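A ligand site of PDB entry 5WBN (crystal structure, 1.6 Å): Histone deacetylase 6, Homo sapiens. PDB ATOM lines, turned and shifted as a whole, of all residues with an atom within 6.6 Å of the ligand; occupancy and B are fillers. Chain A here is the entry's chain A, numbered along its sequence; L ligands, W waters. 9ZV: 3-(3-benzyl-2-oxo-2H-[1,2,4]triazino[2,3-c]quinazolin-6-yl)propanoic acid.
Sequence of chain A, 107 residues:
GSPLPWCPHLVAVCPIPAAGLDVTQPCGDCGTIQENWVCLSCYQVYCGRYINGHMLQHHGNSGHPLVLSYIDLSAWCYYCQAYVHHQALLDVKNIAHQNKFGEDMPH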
ATOM      1  N   GLU A  35      10.958  18.423  34.989  1.00  0.00           N
ATOM      2  CA  GLU A  35      10.439  18.610  33.619  1.00  0.00           C
ATOM      3  C   GLU A  35      10.776  19.962  33.057  1.00  0.00           C
ATOM      4  O   GLU A  35       9.996  20.551  32.323  1.00  0.00           O
ATOM      5  CB  GLU A  35       8.945  18.307  33.519  1.00  0.00           C
ATOM      6  CG  GLU A  35       8.714  16.811  33.722  1.00  0.00           C
ATOM      7  CD  GLU A  35       7.357  16.477  34.190  1.00  0.00           C
ATOM      8  OE1 GLU A  35       7.283  15.542  35.023  1.00  0.00           O
ATOM      9  OE2 GLU A  35       6.370  17.127  33.786  1.00  0.00           O
ATOM     10  N   TRP A  37      12.886  22.521  30.556  1.00  0.00           N
ATOM     11  CA  TRP A  37      13.376  22.620  29.203  1.00  0.00           C
ATOM     12  C   TRP A  37      14.367  23.781  29.189  1.00  0.00           C
ATOM     13  O   TRP A  37      14.329  24.731  30.040  1.00  0.00           O
ATOM     14  CB  TRP A  37      12.241  22.918  28.228  1.00  0.00           C
ATOM     15  CG  TRP A  37      11.201  21.836  28.133  1.00  0.00           C
ATOM     16  CD1 TRP A  37      10.356  21.446  29.119  1.00  0.00           C
ATOM     17  CD2 TRP A  37      10.887  21.011  26.973  1.00  0.00           C
ATOM     18  NE1 TRP A  37       9.514  20.416  28.651  1.00  0.00           N
ATOM     19  CE2 TRP A  37       9.842  20.124  27.359  1.00  0.00           C
ATOM     20  CE3 TRP A  37      11.395  20.926  25.670  1.00  0.00           C
ATOM     21  CZ2 TRP A  37       9.280  19.170  26.475  1.00  0.00           C
ATOM     22  CZ3 TRP A  37      10.852  19.983  24.775  1.00  0.00           C
ATOM     23  CH2 TRP A  37       9.769  19.110  25.211  1.00  0.00           C
ATOM     24  N   CYS A  47      10.125  25.519  33.098  1.00  0.00           N
ATOM     25  CA  CYS A  47       9.447  24.239  33.159  1.00  0.00           C
ATOM     26  C   CYS A  47       8.461  23.948  32.011  1.00  0.00           C
ATOM     27  O   CYS A  47       7.921  24.854  31.332  1.00  0.00           O
ATOM     28  CB  CYS A  47       8.776  24.111  34.519  1.00  0.00           C
ATOM     29  SG  CYS A  47       7.497  25.325  34.775  1.00  0.00           S
ATOM     30  N   GLY A  48       8.233  22.654  31.805  1.00  0.00           N
ATOM     31  CA  GLY A  48       7.335  22.194  30.756  1.00  0.00           C
ATOM     32  C   GLY A  48       5.867  22.386  31.083  1.00  0.00           C
ATOM     33  O   GLY A  48       5.496  22.746  32.202  1.00  0.00           O
ATOM     34  N   ARG A  49       5.022  22.086  30.097  1.00  0.00           N
ATOM     35  CA  ARG A  49       3.623  22.447  30.232  1.00  0.00           C
ATOM     36  C   ARG A  49       2.856  21.593  31.239  1.00  0.00           C
ATOM     37  O   ARG A  49       1.778  21.986  31.638  1.00  0.00           O
ATOM     38  CB  ARG A  49       2.904  22.506  28.862  1.00  0.00           C
ATOM     39  CG  ARG A  49       2.720  21.195  28.119  1.00  0.00           C
ATOM     40  CD  ARG A  49       2.020  21.475  26.785  1.00  0.00           C
ATOM     41  NE  ARG A  49       1.757  20.297  25.946  1.00  0.00           N
ATOM     42  CZ  ARG A  49       0.834  20.228  24.974  1.00  0.00           C
ATOM     43  NH1 ARG A  49       0.680  19.094  24.293  1.00  0.00           N
ATOM     44  NH2 ARG A  49       0.021  21.255  24.679  1.00  0.00           N
ATOM     45  N   TYR A  50       3.398  20.459  31.623  1.00  0.00           N
ATOM     46  CA  TYR A  50       2.784  19.609  32.641  1.00  0.00           C
ATOM     47  C   TYR A  50       3.209  20.027  34.046  1.00  0.00           C
ATOM     48  O   TYR A  50       2.613  19.528  34.994  1.00  0.00           O
ATOM     49  CB  TYR A  50       2.928  18.097  32.355  1.00  0.00           C
ATOM     50  CG  TYR A  50       2.297  17.777  31.019  1.00  0.00           C
ATOM     51  CD1 TYR A  50       0.928  17.898  30.832  1.00  0.00           C
ATOM     52  CD2 TYR A  50       3.059  17.437  29.923  1.00  0.00           C
ATOM     53  CE1 TYR A  50       0.332  17.672  29.602  1.00  0.00           C
ATOM     54  CE2 TYR A  50       2.464  17.211  28.676  1.00  0.00           C
ATOM     55  CZ  TYR A  50       1.099  17.339  28.512  1.00  0.00           C
ATOM     56  OH  TYR A  50       0.512  17.162  27.286  1.00  0.00           O
ATOM     57  N   GLY A  53       4.303  25.451  32.992  1.00  0.00           N
ATOM     58  CA  GLY A  53       4.222  26.029  31.634  1.00  0.00           C
ATOM     59  C   GLY A  53       5.074  27.269  31.443  1.00  0.00           C
ATOM     60  O   GLY A  53       4.787  28.094  30.580  1.00  0.00           O
ATOM     61  N   HIS A  54       6.147  27.403  32.208  1.00  0.00           N
ATOM     62  CA  HIS A  54       6.985  28.599  32.117  1.00  0.00           C
ATOM     63  C   HIS A  54       7.771  28.653  30.840  1.00  0.00           C
ATOM     64  O   HIS A  54       8.028  29.762  30.357  1.00  0.00           O
ATOM     65  CB  HIS A  54       7.840  28.815  33.339  1.00  0.00           C
ATOM     66  CG  HIS A  54       7.015  29.209  34.510  1.00  0.00           C
ATOM     67  ND1 HIS A  54       7.055  28.550  35.732  1.00  0.00           N
ATOM     68  CD2 HIS A  54       6.080  30.185  34.629  1.00  0.00           C
ATOM     69  CE1 HIS A  54       6.151  29.099  36.528  1.00  0.00           C
ATOM     70  NE2 HIS A  54       5.564  30.113  35.899  1.00  0.00           N
ATOM     71  N   MET A  55       8.117  27.503  30.264  1.00  0.00           N
ATOM     72  CA  MET A  55       8.783  27.549  28.972  1.00  0.00           C
ATOM     73  C   MET A  55       7.809  28.029  27.872  1.00  0.00           C
ATOM     74  O   MET A  55       8.174  28.829  26.998  1.00  0.00           O
ATOM     75  CB  MET A  55       9.450  26.240  28.537  1.00  0.00           C
ATOM     76  CG  MET A  55      10.276  26.485  27.315  1.00  0.00           C
ATOM     77  SD  MET A  55      11.560  27.766  27.536  1.00  0.00           S
ATOM     78  CE  MET A  55      12.862  26.790  28.291  1.00  0.00           C
ATOM     79  N   LEU A  56       6.591  27.514  27.873  1.00  0.00           N
ATOM     80  CA  LEU A  56       5.558  28.038  26.948  1.00  0.00           C
ATOM     81  C   LEU A  56       5.323  29.548  27.116  1.00  0.00           C
ATOM     82  O   LEU A  56       5.197  30.291  26.113  1.00  0.00           O
ATOM     83  CB  LEU A  56       4.264  27.231  27.084  1.00  0.00           C
ATOM     84  CG  LEU A  56       3.102  27.571  26.170  1.00  0.00           C
ATOM     85  CD1 LEU A  56       3.510  27.560  24.698  1.00  0.00           C
ATOM     86  CD2 LEU A  56       1.965  26.559  26.426  1.00  0.00           C
ATOM     87  N   GLN A  57       5.346  30.011  28.354  1.00  0.00           N
ATOM     88  CA  GLN A  57       5.282  31.442  28.636  1.00  0.00           C
ATOM     89  C   GLN A  57       6.471  32.183  28.060  1.00  0.00           C
ATOM     90  O   GLN A  57       6.320  33.255  27.478  1.00  0.00           O
ATOM     91  CB  GLN A  57       5.240  31.675  30.120  1.00  0.00           C
ATOM     92  CG  GLN A  57       5.061  33.105  30.520  1.00  0.00           C
ATOM     93  CD  GLN A  57       4.963  33.146  32.036  1.00  0.00           C
ATOM     94  OE1 GLN A  57       3.957  32.803  32.562  1.00  0.00           O
ATOM     95  NE2 GLN A  57       6.054  33.437  32.701  1.00  0.00           N
ATOM     96  N   VAL A  67      12.845  24.541  21.940  1.00  0.00           N
ATOM     97  CA  VAL A  67      13.223  24.221  23.289  1.00  0.00           C
ATOM     98  C   VAL A  67      13.609  22.762  23.379  1.00  0.00           C
ATOM     99  O   VAL A  67      13.034  21.924  22.650  1.00  0.00           O
ATOM    100  CB  VAL A  67      12.106  24.545  24.252  1.00  0.00           C
ATOM    101  CG1 VAL A  67      11.887  26.059  24.240  1.00  0.00           C
ATOM    102  CG2 VAL A  67      10.808  23.815  23.886  1.00  0.00           C
ATOM    103  N   ASP A  72      14.211  14.024  28.193  1.00  0.00           N
ATOM    104  CA  ASP A  72      14.558  13.043  27.157  1.00  0.00           C
ATOM    105  C   ASP A  72      15.332  13.618  26.003  1.00  0.00           C
ATOM    106  O   ASP A  72      15.572  12.916  25.018  1.00  0.00           O
ATOM    107  CB  ASP A  72      13.304  12.323  26.653  1.00  0.00           C
ATOM    108  CG  ASP A  72      12.415  13.204  25.795  1.00  0.00           C
ATOM    109  OD1 ASP A  72      12.646  14.396  25.660  1.00  0.00           O
ATOM    110  OD2 ASP A  72      11.471  12.643  25.213  1.00  0.00           O
ATOM    111  N   SER A  74      14.590  15.638  23.697  1.00  0.00           N
ATOM    112  CA  SER A  74      13.896  15.922  22.443  1.00  0.00           C
ATOM    113  C   SER A  74      13.794  17.437  22.297  1.00  0.00           C
ATOM    114  O   SER A  74      13.848  18.170  23.302  1.00  0.00           O
ATOM    115  CB  SER A  74      12.525  15.245  22.413  1.00  0.00           C
ATOM    116  OG  SER A  74      11.710  15.688  23.461  1.00  0.00           O
ATOM    117  N   TRP A  76      11.454  20.452  20.693  1.00  0.00           N
ATOM    118  CA  TRP A  76      10.118  20.789  20.213  1.00  0.00           C
ATOM    119  C   TRP A  76      10.131  22.193  19.643  1.00  0.00           C
ATOM    120  O   TRP A  76      10.720  23.126  20.314  1.00  0.00           O
ATOM    121  CB  TRP A  76       9.155  20.736  21.385  1.00  0.00           C
ATOM    122  CG  TRP A  76       7.766  21.014  21.022  1.00  0.00           C
ATOM    123  CD1 TRP A  76       7.095  22.181  21.169  1.00  0.00           C
ATOM    124  CD2 TRP A  76       6.857  20.091  20.390  1.00  0.00           C
ATOM    125  NE1 TRP A  76       5.804  22.024  20.721  1.00  0.00           N
ATOM    126  CE2 TRP A  76       5.643  20.777  20.202  1.00  0.00           C
ATOM    127  CE3 TRP A  76       6.944  18.750  19.977  1.00  0.00           C
ATOM    128  CZ2 TRP A  76       4.524  20.174  19.639  1.00  0.00           C
ATOM    129  CZ3 TRP A  76       5.834  18.160  19.425  1.00  0.00           C
ATOM    130  CH2 TRP A  76       4.647  18.873  19.271  1.00  0.00           C
ATOM    131  N   TYR A  78       7.676  25.183  18.881  1.00  0.00           N
ATOM    132  CA  TYR A  78       6.343  25.667  19.237  1.00  0.00           C
ATOM    133  C   TYR A  78       5.569  26.117  17.989  1.00  0.00           C
ATOM    134  O   TYR A  78       4.394  25.914  17.913  1.00  0.00           O
ATOM    135  CB  TYR A  78       6.462  26.820  20.246  1.00  0.00           C
ATOM    136  CG  TYR A  78       6.854  26.429  21.634  1.00  0.00           C
ATOM    137  CD1 TYR A  78       5.986  25.654  22.413  1.00  0.00           C
ATOM    138  CD2 TYR A  78       8.056  26.823  22.204  1.00  0.00           C
ATOM    139  CE1 TYR A  78       6.298  25.309  23.703  1.00  0.00           C
ATOM    140  CE2 TYR A  78       8.362  26.473  23.506  1.00  0.00           C
ATOM    141  CZ  TYR A  78       7.489  25.747  24.248  1.00  0.00           C
ATOM    142  OH  TYR A  78       7.811  25.430  25.548  1.00  0.00           O
ATOM    143  N   GLN A  81       4.813  22.879  15.829  1.00  0.00           N
ATOM    144  CA  GLN A  81       4.084  21.926  16.640  1.00  0.00           C
ATOM    145  C   GLN A  81       4.551  20.488  16.315  1.00  0.00           C
ATOM    146  O   GLN A  81       3.770  19.564  15.971  1.00  0.00           O
ATOM    147  CB  GLN A  81       2.583  22.051  16.379  1.00  0.00           C
ATOM    148  CG  GLN A  81       2.066  23.455  16.323  1.00  0.00           C
ATOM    149  CD  GLN A  81       0.579  23.480  15.957  1.00  0.00           C
ATOM    150  OE1 GLN A  81      -0.243  22.992  16.723  1.00  0.00           O
ATOM    151  NE2 GLN A  81       0.240  24.062  14.793  1.00  0.00           N
ATOM    152  N   ALA A  82       5.846  20.328  16.380  1.00  0.00           N
ATOM    153  CA  ALA A  82       6.450  19.055  16.097  1.00  0.00           C
ATOM    154  C   ALA A  82       7.779  18.940  16.757  1.00  0.00           C
ATOM    155  O   ALA A  82       8.464  19.946  17.081  1.00  0.00           O
ATOM    156  CB  ALA A  82       6.625  18.870  14.603  1.00  0.00           C
ATOM    157  N   TYR A  83       8.165  17.694  16.945  1.00  0.00           N
ATOM    158  CA  TYR A  83       9.522  17.419  17.296  1.00  0.00           C
ATOM    159  C   TYR A  83      10.356  17.591  16.066  1.00  0.00           C
ATOM    160  O   TYR A  83       9.878  17.357  14.945  1.00  0.00           O
ATOM    161  CB  TYR A  83       9.688  15.979  17.689  1.00  0.00           C
ATOM    162  CG  TYR A  83       9.181  15.581  19.028  1.00  0.00           C
ATOM    163  CD1 TYR A  83       9.687  16.141  20.173  1.00  0.00           C
ATOM    164  CD2 TYR A  83       8.316  14.518  19.140  1.00  0.00           C
ATOM    165  CE1 TYR A  83       9.283  15.671  21.428  1.00  0.00           C
ATOM    166  CE2 TYR A  83       7.924  14.037  20.360  1.00  0.00           C
ATOM    167  CZ  TYR A  83       8.441  14.589  21.507  1.00  0.00           C
ATOM    168  OH  TYR A  83       7.998  14.085  22.726  1.00  0.00           O
HETATM  169  C13 9ZV L   1       6.167  16.516  22.935  1.00  0.00           C
HETATM  170  N2  9ZV L   1       5.767  18.803  23.468  1.00  0.00           N
HETATM  171  C17 9ZV L   1       4.993  14.016  26.229  1.00  0.00           C
HETATM  172  C11 9ZV L   1       3.963  17.685  22.265  1.00  0.00           C
HETATM  173  C9  9ZV L   1       2.999  23.504  23.445  1.00  0.00           C
HETATM  174  C8  9ZV L   1       1.802  23.652  22.759  1.00  0.00           C
HETATM  175  N1  9ZV L   1       3.256  18.833  22.216  1.00  0.00           N
HETATM  176  O1  9ZV L   1       6.420  23.835  26.983  1.00  0.00           O
HETATM  177  O2  9ZV L   1       3.517  16.630  21.784  1.00  0.00           O
HETATM  178  C1  9ZV L   1       7.334  22.149  25.517  1.00  0.00           C
HETATM  179  C2  9ZV L   1       6.819  20.905  24.789  1.00  0.00           C
HETATM  180  C3  9ZV L   1       5.471  21.045  24.168  1.00  0.00           C
HETATM  181  C4  9ZV L   1       3.649  22.275  23.462  1.00  0.00           C
HETATM  182  C5  9ZV L   1       3.089  21.187  22.759  1.00  0.00           C
HETATM  183  C6  9ZV L   1       1.898  21.375  22.036  1.00  0.00           C
HETATM  184  C7  9ZV L   1       1.264  22.603  22.043  1.00  0.00           C
HETATM  185  C10 9ZV L   1       3.787  19.919  22.803  1.00  0.00           C
HETATM  186  C12 9ZV L   1       5.299  17.733  22.900  1.00  0.00           C
HETATM  187  C14 9ZV L   1       5.762  15.642  24.095  1.00  0.00           C
HETATM  188  C19 9ZV L   1       5.204  14.377  23.875  1.00  0.00           C
HETATM  189  C18 9ZV L   1       4.831  13.573  24.939  1.00  0.00           C
HETATM  190  C16 9ZV L   1       5.547  15.253  26.468  1.00  0.00           C
HETATM  191  C15 9ZV L   1       5.925  16.064  25.409  1.00  0.00           C
HETATM  192  N3  9ZV L   1       4.986  19.908  23.516  1.00  0.00           N
HETATM  193  C   9ZV L   1       6.538  22.632  26.697  1.00  0.00           C
HETATM  194  O   9ZV L   1       5.954  21.685  27.397  1.00  0.00           O
HETATM  195  N   9ZV L   1       4.849  22.171  24.180  1.00  0.00           N
HETATM  196  O   HOH W   1       3.747  18.455  25.758  1.00  0.00           O
HETATM  197  O   HOH W   2       3.500  23.768  19.752  1.00  0.00           O
HETATM  198  O   HOH W   3       6.044  25.134  29.245  1.00  0.00           O
HETATM  199  O   HOH W   4       1.070  22.816  19.028  1.00  0.00           O
HETATM  200  O   HOH W   5       5.736  19.078  27.629  1.00  0.00           O
HETATM  201  O   HOH W   6       3.838  14.522  20.060  1.00  0.00           O
HETATM  202  O   HOH W   7      -0.428  24.077  25.384  1.00  0.00           O
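The side-chain hydroxyl (OH) of Tyr 78 sits at hydrogen-bond distance from the backbone NH (N) of Leu 56 (3.4 Å).
The backbone NH (N) of Gly 48 is in hydrogen-bond range of the backbone carbonyl oxygen (O) of Glu 35.
The backbone carbonyl oxygen of Gly 48 sits at hydrogen-bond distance from the backbone NH of Gly 53 (3.1 Å).
The backbone NH (N) of Trp 76 lies within hydrogen-bond range of the backbone carbonyl oxygen (O) of Val 67, 2.9 Å away.
The guanidinium group (NH1) of Arg 49 is in hydrogen-bond range of a nitrogen (N1) of the ligand (3.3 Å).
N of Arg 49 lies within hydrogen-bond range of O of the ligand (2.9 Å).
An oxygen (O1) of the ligand is in hydrogen-bond range of the side-chain hydroxyl (OH) of Tyr 78 (2.6 Å).
Residues that only touch the ligand: Trp 37, Gly 48, Leu 56, Trp 76 and Tyr 83.
The nearest printed residue that does not touch the ligand is Met 55 (4.2 Å).
Water W1 bridges the guanidinium group (NE) of Arg 49 (2.7 Å) and a nitrogen (N2) of the ligand (3.1 Å).
Water W2 bridges the backbone carbonyl oxygen of Tyr 78 (3.0 Å) and the indole nitrogen of Trp 76 (3.0 Å).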
